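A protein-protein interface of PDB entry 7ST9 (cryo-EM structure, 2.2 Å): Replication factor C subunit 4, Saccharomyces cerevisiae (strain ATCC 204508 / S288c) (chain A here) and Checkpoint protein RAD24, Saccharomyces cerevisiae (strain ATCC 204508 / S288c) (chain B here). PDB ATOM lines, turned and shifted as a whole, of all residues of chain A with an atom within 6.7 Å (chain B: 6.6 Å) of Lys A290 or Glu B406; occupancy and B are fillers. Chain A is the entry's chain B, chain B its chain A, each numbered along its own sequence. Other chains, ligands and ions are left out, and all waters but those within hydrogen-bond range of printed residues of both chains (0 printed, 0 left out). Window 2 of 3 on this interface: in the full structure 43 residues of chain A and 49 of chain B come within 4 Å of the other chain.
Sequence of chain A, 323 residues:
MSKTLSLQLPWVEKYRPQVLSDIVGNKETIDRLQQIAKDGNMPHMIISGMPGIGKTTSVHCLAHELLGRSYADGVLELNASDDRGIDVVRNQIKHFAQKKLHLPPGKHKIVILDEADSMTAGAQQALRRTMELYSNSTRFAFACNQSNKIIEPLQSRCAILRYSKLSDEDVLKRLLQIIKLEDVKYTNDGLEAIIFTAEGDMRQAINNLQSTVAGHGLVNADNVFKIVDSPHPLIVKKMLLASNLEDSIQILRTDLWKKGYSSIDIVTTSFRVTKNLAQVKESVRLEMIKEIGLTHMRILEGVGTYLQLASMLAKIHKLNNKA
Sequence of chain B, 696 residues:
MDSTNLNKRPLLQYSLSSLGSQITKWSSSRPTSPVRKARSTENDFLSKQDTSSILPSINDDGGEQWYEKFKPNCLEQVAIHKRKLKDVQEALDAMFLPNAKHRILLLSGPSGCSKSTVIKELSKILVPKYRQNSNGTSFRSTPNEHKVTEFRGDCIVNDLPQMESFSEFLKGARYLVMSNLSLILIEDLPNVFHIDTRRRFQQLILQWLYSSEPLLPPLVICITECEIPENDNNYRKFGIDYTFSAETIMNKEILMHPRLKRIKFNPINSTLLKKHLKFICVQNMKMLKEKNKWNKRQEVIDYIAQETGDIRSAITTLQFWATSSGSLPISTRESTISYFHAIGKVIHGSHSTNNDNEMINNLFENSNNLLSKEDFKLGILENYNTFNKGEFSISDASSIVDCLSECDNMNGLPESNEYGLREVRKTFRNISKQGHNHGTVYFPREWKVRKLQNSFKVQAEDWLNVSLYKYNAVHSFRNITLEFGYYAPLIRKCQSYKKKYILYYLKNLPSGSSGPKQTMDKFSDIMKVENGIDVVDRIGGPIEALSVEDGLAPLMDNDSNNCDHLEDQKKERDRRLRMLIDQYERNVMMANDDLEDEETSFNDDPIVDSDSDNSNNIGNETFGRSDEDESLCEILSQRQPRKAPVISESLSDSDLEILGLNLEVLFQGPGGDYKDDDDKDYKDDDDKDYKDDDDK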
ATOM      1  N   ARG A 285      17.010  -5.307   9.575  1.00  0.00           N
ATOM      2  CA  ARG A 285      15.719  -4.945  10.150  1.00  0.00           C
ATOM      3  C   ARG A 285      15.330  -3.517   9.784  1.00  0.00           C
ATOM      4  O   ARG A 285      14.179  -3.257   9.412  1.00  0.00           O
ATOM      5  CB  ARG A 285      15.761  -5.115  11.668  1.00  0.00           C
ATOM      6  CG  ARG A 285      14.423  -4.912  12.359  1.00  0.00           C
ATOM      7  CD  ARG A 285      14.611  -4.344  13.751  1.00  0.00           C
ATOM      8  NE  ARG A 285      15.524  -5.156  14.546  1.00  0.00           N
ATOM      9  CZ  ARG A 285      15.234  -6.356  15.028  1.00  0.00           C
ATOM     10  NH1 ARG A 285      14.052  -6.914  14.825  1.00  0.00           N
ATOM     11  NH2 ARG A 285      16.151  -7.012  15.732  1.00  0.00           N
ATOM     12  N   LEU A 286      16.271  -2.576   9.885  1.00  0.00           N
ATOM     13  CA  LEU A 286      15.940  -1.189   9.580  1.00  0.00           C
ATOM     14  C   LEU A 286      15.679  -1.002   8.089  1.00  0.00           C
ATOM     15  O   LEU A 286      14.804  -0.218   7.702  1.00  0.00           O
ATOM     16  CB  LEU A 286      17.049  -0.253  10.071  1.00  0.00           C
ATOM     17  CG  LEU A 286      18.324  -0.101   9.240  1.00  0.00           C
ATOM     18  CD1 LEU A 286      18.220   1.076   8.287  1.00  0.00           C
ATOM     19  CD2 LEU A 286      19.526   0.068  10.155  1.00  0.00           C
ATOM     20  N   GLU A 287      16.409  -1.723   7.234  1.00  0.00           N
ATOM     21  CA  GLU A 287      16.119  -1.653   5.804  1.00  0.00           C
ATOM     22  C   GLU A 287      14.729  -2.205   5.494  1.00  0.00           C
ATOM     23  O   GLU A 287      13.994  -1.639   4.672  1.00  0.00           O
ATOM     24  CB  GLU A 287      17.188  -2.408   5.013  1.00  0.00           C
ATOM     25  CG  GLU A 287      18.567  -1.766   5.053  1.00  0.00           C
ATOM     26  CD  GLU A 287      18.564  -0.332   4.561  1.00  0.00           C
ATOM     27  OE1 GLU A 287      17.673   0.024   3.763  1.00  0.00           O
ATOM     28  OE2 GLU A 287      19.456   0.440   4.974  1.00  0.00           O
ATOM     29  N   MET A 288      14.352  -3.311   6.139  1.00  0.00           N
ATOM     30  CA  MET A 288      13.007  -3.849   5.955  1.00  0.00           C
ATOM     31  C   MET A 288      11.953  -2.862   6.434  1.00  0.00           C
ATOM     32  O   MET A 288      10.902  -2.707   5.802  1.00  0.00           O
ATOM     33  CB  MET A 288      12.859  -5.182   6.689  1.00  0.00           C
ATOM     34  CG  MET A 288      13.803  -6.272   6.216  1.00  0.00           C
ATOM     35  SD  MET A 288      14.023  -7.574   7.443  1.00  0.00           S
ATOM     36  CE  MET A 288      12.325  -8.033   7.771  1.00  0.00           C
ATOM     37  N   ILE A 289      12.208  -2.194   7.562  1.00  0.00           N
ATOM     38  CA  ILE A 289      11.274  -1.185   8.050  1.00  0.00           C
ATOM     39  C   ILE A 289      11.131  -0.062   7.032  1.00  0.00           C
ATOM     40  O   ILE A 289      10.026   0.433   6.783  1.00  0.00           O
ATOM     41  CB  ILE A 289      11.727  -0.652   9.422  1.00  0.00           C
ATOM     42  CG1 ILE A 289      11.482  -1.700  10.509  1.00  0.00           C
ATOM     43  CG2 ILE A 289      10.997   0.639   9.759  1.00  0.00           C
ATOM     44  CD1 ILE A 289      12.296  -1.480  11.763  1.00  0.00           C
ATOM     45  N   LYS A 290      12.246   0.365   6.437  1.00  0.00           N
ATOM     46  CA  LYS A 290      12.191   1.419   5.427  1.00  0.00           C
ATOM     47  C   LYS A 290      11.343   0.992   4.232  1.00  0.00           C
ATOM     48  O   LYS A 290      10.497   1.755   3.747  1.00  0.00           O
ATOM     49  CB  LYS A 290      13.609   1.780   4.981  1.00  0.00           C
ATOM     50  CG  LYS A 290      13.691   2.955   4.019  1.00  0.00           C
ATOM     51  CD  LYS A 290      14.971   2.906   3.202  1.00  0.00           C
ATOM     52  CE  LYS A 290      15.062   4.073   2.235  1.00  0.00           C
ATOM     53  NZ  LYS A 290      16.240   3.959   1.334  1.00  0.00           N
ATOM     54  N   GLU A 291      11.564  -0.228   3.739  1.00  0.00           N
ATOM     55  CA  GLU A 291      10.791  -0.701   2.592  1.00  0.00           C
ATOM     56  C   GLU A 291       9.310  -0.813   2.933  1.00  0.00           C
ATOM     57  O   GLU A 291       8.444  -0.442   2.127  1.00  0.00           O
ATOM     58  CB  GLU A 291      11.334  -2.047   2.108  1.00  0.00           C
ATOM     59  CG  GLU A 291      12.755  -1.991   1.559  1.00  0.00           C
ATOM     60  CD  GLU A 291      12.913  -0.991   0.428  1.00  0.00           C
ATOM     61  OE1 GLU A 291      11.889  -0.595  -0.169  1.00  0.00           O
ATOM     62  OE2 GLU A 291      14.061  -0.596   0.137  1.00  0.00           O
ATOM     63  N   ILE A 292       8.998  -1.317   4.129  1.00  0.00           N
ATOM     64  CA  ILE A 292       7.606  -1.430   4.550  1.00  0.00           C
ATOM     65  C   ILE A 292       6.966  -0.053   4.634  1.00  0.00           C
ATOM     66  O   ILE A 292       5.811   0.135   4.240  1.00  0.00           O
ATOM     67  CB  ILE A 292       7.513  -2.183   5.891  1.00  0.00           C
ATOM     68  CG1 ILE A 292       7.851  -3.663   5.694  1.00  0.00           C
ATOM     69  CG2 ILE A 292       6.124  -2.034   6.493  1.00  0.00           C
ATOM     70  CD1 ILE A 292       8.242  -4.376   6.970  1.00  0.00           C
ATOM     71  N   GLY A 293       7.702   0.932   5.152  1.00  0.00           N
ATOM     72  CA  GLY A 293       7.165   2.280   5.229  1.00  0.00           C
ATOM     73  C   GLY A 293       6.909   2.884   3.862  1.00  0.00           C
ATOM     74  O   GLY A 293       5.901   3.562   3.653  1.00  0.00           O
ATOM     75  N   LEU A 294       7.818   2.653   2.913  1.00  0.00           N
ATOM     76  CA  LEU A 294       7.596   3.148   1.557  1.00  0.00           C
ATOM     77  C   LEU A 294       6.355   2.509   0.937  1.00  0.00           C
ATOM     78  O   LEU A 294       5.538   3.194   0.304  1.00  0.00           O
ATOM     79  CB  LEU A 294       8.829   2.882   0.691  1.00  0.00           C
ATOM     80  CG  LEU A 294      10.090   3.667   1.064  1.00  0.00           C
ATOM     81  CD1 LEU A 294      11.309   3.098   0.352  1.00  0.00           C
ATOM     82  CD2 LEU A 294       9.928   5.147   0.746  1.00  0.00           C
ATOM     83  N   THR A 295       6.191   1.196   1.120  1.00  0.00           N
ATOM     84  CA  THR A 295       5.001   0.528   0.602  1.00  0.00           C
ATOM     85  C   THR A 295       3.737   1.062   1.269  1.00  0.00           C
ATOM     86  O   THR A 295       2.703   1.232   0.613  1.00  0.00           O
ATOM     87  CB  THR A 295       5.113  -0.983   0.801  1.00  0.00           C
ATOM     88  OG1 THR A 295       6.244  -1.479   0.076  1.00  0.00           O
ATOM     89  CG2 THR A 295       3.854  -1.687   0.312  1.00  0.00           C
ATOM     90  N   LEU A 319      17.176  -7.373   0.440  1.00  0.00           N
ATOM     91  CA  LEU A 319      17.856  -6.948   1.660  1.00  0.00           C
ATOM     92  C   LEU A 319      18.464  -8.140   2.386  1.00  0.00           C
ATOM     93  O   LEU A 319      19.579  -8.053   2.913  1.00  0.00           O
ATOM     94  CB  LEU A 319      16.882  -6.204   2.572  1.00  0.00           C
ATOM     95  CG  LEU A 319      16.366  -4.864   2.047  1.00  0.00           C
ATOM     96  CD1 LEU A 319      15.266  -4.326   2.949  1.00  0.00           C
ATOM     97  CD2 LEU A 319      17.504  -3.864   1.921  1.00  0.00           C
ATOM     98  N   LYS B 377      14.023  15.106  15.107  1.00  0.00           N
ATOM     99  CA  LYS B 377      14.861  14.887  13.934  1.00  0.00           C
ATOM    100  C   LYS B 377      15.809  16.059  13.716  1.00  0.00           C
ATOM    101  O   LYS B 377      16.971  15.865  13.343  1.00  0.00           O
ATOM    102  CB  LYS B 377      13.992  14.660  12.697  1.00  0.00           C
ATOM    103  CG  LYS B 377      14.071  13.247  12.134  1.00  0.00           C
ATOM    104  CD  LYS B 377      12.811  12.865  11.365  1.00  0.00           C
ATOM    105  CE  LYS B 377      12.586  13.753  10.146  1.00  0.00           C
ATOM    106  NZ  LYS B 377      13.509  13.415   9.028  1.00  0.00           N
ATOM    107  N   VAL B 401      22.738  11.871   7.270  1.00  0.00           N
ATOM    108  CA  VAL B 401      21.952  12.974   6.729  1.00  0.00           C
ATOM    109  C   VAL B 401      21.075  12.494   5.579  1.00  0.00           C
ATOM    110  O   VAL B 401      19.939  12.954   5.417  1.00  0.00           O
ATOM    111  CB  VAL B 401      22.871  14.133   6.300  1.00  0.00           C
ATOM    112  CG1 VAL B 401      22.050  15.269   5.712  1.00  0.00           C
ATOM    113  CG2 VAL B 401      23.683  14.635   7.484  1.00  0.00           C
ATOM    114  N   ASP B 402      21.583  11.574   4.755  1.00  0.00           N
ATOM    115  CA  ASP B 402      20.772  11.025   3.676  1.00  0.00           C
ATOM    116  C   ASP B 402      19.573  10.269   4.228  1.00  0.00           C
ATOM    117  O   ASP B 402      18.461  10.375   3.694  1.00  0.00           O
ATOM    118  CB  ASP B 402      21.623  10.111   2.796  1.00  0.00           C
ATOM    119  CG  ASP B 402      20.838   9.511   1.646  1.00  0.00           C
ATOM    120  OD1 ASP B 402      19.985  10.219   1.073  1.00  0.00           O
ATOM    121  OD2 ASP B 402      21.074   8.331   1.314  1.00  0.00           O
ATOM    122  N   CYS B 403      19.776   9.498   5.299  1.00  0.00           N
ATOM    123  CA  CYS B 403      18.656   8.800   5.918  1.00  0.00           C
ATOM    124  C   CYS B 403      17.633   9.782   6.474  1.00  0.00           C
ATOM    125  O   CYS B 403      16.423   9.573   6.337  1.00  0.00           O
ATOM    126  CB  CYS B 403      19.161   7.870   7.018  1.00  0.00           C
ATOM    127  SG  CYS B 403      17.836   7.092   7.955  1.00  0.00           S
ATOM    128  N   LEU B 404      18.099  10.858   7.112  1.00  0.00           N
ATOM    129  CA  LEU B 404      17.165  11.860   7.624  1.00  0.00           C
ATOM    130  C   LEU B 404      16.386  12.518   6.487  1.00  0.00           C
ATOM    131  O   LEU B 404      15.176  12.755   6.605  1.00  0.00           O
ATOM    132  CB  LEU B 404      17.920  12.911   8.439  1.00  0.00           C
ATOM    133  CG  LEU B 404      18.618  12.396   9.702  1.00  0.00           C
ATOM    134  CD1 LEU B 404      19.531  13.466  10.283  1.00  0.00           C
ATOM    135  CD2 LEU B 404      17.606  11.937  10.739  1.00  0.00           C
ATOM    136  N   SER B 405      17.063  12.817   5.377  1.00  0.00           N
ATOM    137  CA  SER B 405      16.383  13.402   4.226  1.00  0.00           C
ATOM    138  C   SER B 405      15.331  12.450   3.670  1.00  0.00           C
ATOM    139  O   SER B 405      14.221  12.872   3.323  1.00  0.00           O
ATOM    140  CB  SER B 405      17.404  13.766   3.148  1.00  0.00           C
ATOM    141  OG  SER B 405      16.772  14.265   1.984  1.00  0.00           O
ATOM    142  N   GLU B 406      15.660  11.160   3.577  1.00  0.00           N
ATOM    143  CA  GLU B 406      14.680  10.182   3.115  1.00  0.00           C
ATOM    144  C   GLU B 406      13.491  10.108   4.065  1.00  0.00           C
ATOM    145  O   GLU B 406      12.340  10.013   3.625  1.00  0.00           O
ATOM    146  CB  GLU B 406      15.335   8.807   2.973  1.00  0.00           C
ATOM    147  CG  GLU B 406      16.223   8.670   1.749  1.00  0.00           C
ATOM    148  CD  GLU B 406      16.220   7.264   1.177  1.00  0.00           C
ATOM    149  OE1 GLU B 406      15.122   6.722   0.932  1.00  0.00           O
ATOM    150  OE2 GLU B 406      17.316   6.702   0.972  1.00  0.00           O
ATOM    151  N   CYS B 407      13.752  10.151   5.373  1.00  0.00           N
ATOM    152  CA  CYS B 407      12.668  10.123   6.348  1.00  0.00           C
ATOM    153  C   CYS B 407      11.767  11.342   6.216  1.00  0.00           C
ATOM    154  O   CYS B 407      10.553  11.243   6.427  1.00  0.00           O
ATOM    155  CB  CYS B 407      13.238  10.043   7.763  1.00  0.00           C
ATOM    156  SG  CYS B 407      13.960   8.446   8.177  1.00  0.00           S
ATOM    157  N   ASP B 408      12.340  12.497   5.872  1.00  0.00           N
ATOM    158  CA  ASP B 408      11.530  13.703   5.718  1.00  0.00           C
ATOM    159  C   ASP B 408      10.509  13.576   4.593  1.00  0.00           C
ATOM    160  O   ASP B 408       9.565  14.372   4.539  1.00  0.00           O
ATOM    161  CB  ASP B 408      12.430  14.913   5.461  1.00  0.00           C
ATOM    162  CG  ASP B 408      11.643  16.204   5.325  1.00  0.00           C
ATOM    163  OD1 ASP B 408      10.921  16.567   6.276  1.00  0.00           O
ATOM    164  OD2 ASP B 408      11.740  16.853   4.263  1.00  0.00           O
ATOM    165  N   ASN B 409      10.672  12.603   3.697  1.00  0.00           N
ATOM    166  CA  ASN B 409       9.771  12.404   2.568  1.00  0.00           C
ATOM    167  C   ASN B 409       8.750  11.299   2.823  1.00  0.00           C
ATOM    168  O   ASN B 409       8.155  10.784   1.870  1.00  0.00           O
ATOM    169  CB  ASN B 409      10.577  12.089   1.305  1.00  0.00           C
ATOM    170  CG  ASN B 409      11.103  13.334   0.606  1.00  0.00           C
ATOM    171  OD1 ASN B 409      11.410  13.295  -0.584  1.00  0.00           O
ATOM    172  ND2 ASN B 409      11.220  14.438   1.339  1.00  0.00           N
ATOM    173  N   MET B 410       8.529  10.927   4.084  1.00  0.00           N
ATOM    174  CA  MET B 410       7.673   9.798   4.430  1.00  0.00           C
ATOM    175  C   MET B 410       6.372  10.233   5.096  1.00  0.00           C
ATOM    176  O   MET B 410       5.686   9.407   5.706  1.00  0.00           O
ATOM    177  CB  MET B 410       8.438   8.829   5.329  1.00  0.00           C
ATOM    178  CG  MET B 410       9.604   8.147   4.629  1.00  0.00           C
ATOM    179  SD  MET B 410      10.131   6.616   5.419  1.00  0.00           S
ATOM    180  CE  MET B 410       8.731   5.555   5.079  1.00  0.00           C
ATOM    181  N   GLU B 415       7.101   4.515  10.747  1.00  0.00           N
ATOM    182  CA  GLU B 415       8.209   3.799  10.131  1.00  0.00           C
ATOM    183  C   GLU B 415       9.366   4.739   9.824  1.00  0.00           C
ATOM    184  O   GLU B 415      10.533   4.357   9.952  1.00  0.00           O
ATOM    185  CB  GLU B 415       7.739   3.100   8.855  1.00  0.00           C
ATOM    186  CG  GLU B 415       6.842   1.898   9.098  1.00  0.00           C
ATOM    187  CD  GLU B 415       5.403   2.151   8.691  1.00  0.00           C
ATOM    188  OE1 GLU B 415       4.763   3.044   9.284  1.00  0.00           O
ATOM    189  OE2 GLU B 415       4.913   1.457   7.775  1.00  0.00           O
ATOM    190  N   SER B 416       9.065   5.973   9.417  1.00  0.00           N
ATOM    191  CA  SER B 416      10.125   6.922   9.090  1.00  0.00           C
ATOM    192  C   SER B 416      10.978   7.236  10.314  1.00  0.00           C
ATOM    193  O   SER B 416      12.214   7.200  10.251  1.00  0.00           O
ATOM    194  CB  SER B 416       9.518   8.201   8.513  1.00  0.00           C
ATOM    195  OG  SER B 416       8.942   9.001   9.530  1.00  0.00           O
ATOM    196  N   TYR B 419      13.058   4.167  11.292  1.00  0.00           N
ATOM    197  CA  TYR B 419      14.175   3.974  10.376  1.00  0.00           C
ATOM    198  C   TYR B 419      15.285   4.980  10.646  1.00  0.00           C
ATOM    199  O   TYR B 419      16.465   4.618  10.699  1.00  0.00           O
ATOM    200  CB  TYR B 419      13.669   4.086   8.935  1.00  0.00           C
ATOM    201  CG  TYR B 419      14.744   4.285   7.890  1.00  0.00           C
ATOM    202  CD1 TYR B 419      15.799   3.393   7.767  1.00  0.00           C
ATOM    203  CD2 TYR B 419      14.691   5.360   7.013  1.00  0.00           C
ATOM    204  CE1 TYR B 419      16.777   3.573   6.806  1.00  0.00           C
ATOM    205  CE2 TYR B 419      15.660   5.546   6.049  1.00  0.00           C
ATOM    206  CZ  TYR B 419      16.702   4.650   5.951  1.00  0.00           C
ATOM    207  OH  TYR B 419      17.673   4.831   4.993  1.00  0.00           O
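Among the printed residues, pairs that only touch across the chains: Leu A286 with Tyr B419 (3.2 Å), Ile A289 with Glu B415 (3.8 Å), Lys A290 with Tyr B419 (3.7 Å), Ile A292 with Glu B415 (3.9 Å), Gly A293 with Met B410 (3.5 Å), Gly A293 with Glu B415 (3.5 Å) and Leu A294 with Met B410 (3.7 Å).
The side-chain sulfur (SG) of Cys B403 lies close to the side-chain hydroxyl (OH) of Tyr B419.
NZ of Lys A290 lies within salt-bridge range of OE2 of Glu B406, at 3.0 Å.
Printed residues of chain A that touch a printed residue of chain B: Leu A286, Ile A289, Lys A290, Ile A292, Gly A293 and Leu A294. Hydrophobic or aromatic side chains of chain A that line the printed part of chain B: Leu A286, Ile A289 and Ile A292. Printed residues of chain B that touch a printed residue of chain A: Glu B406, Met B410, Glu B415 and Tyr B419. Hydrophobic or aromatic side chains of chain B that line the printed part of chain A: Met B410 and Tyr B419. Along chain B the printed residues that touch a printed residue of chain A span positions 406 to 419.
Printed residues of chain B within 4 Å of Leu A286: Tyr B419 (3.2 Å). Printed residues of chain B within 4 Å of Ile A289: Glu B415. Printed residues of chain B within 4 Å of Lys A290: Glu B406 (3.0 Å) and Tyr B419 (3.7 Å). Lys B377 touches none of the printed residues of chain A. Asp B402 touches none of the printed residues of chain A. Printed residues of chain A within 4 Å of Glu B406: Lys A290 (3.0 Å). Of the printed residues of chain A, Met B410 touches Gly A293 (3.5 Å) and Leu A294 (3.7 Å). The nearest printed residue of chain B that does not touch Leu A286 is Cys B403 (6.0 Å).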
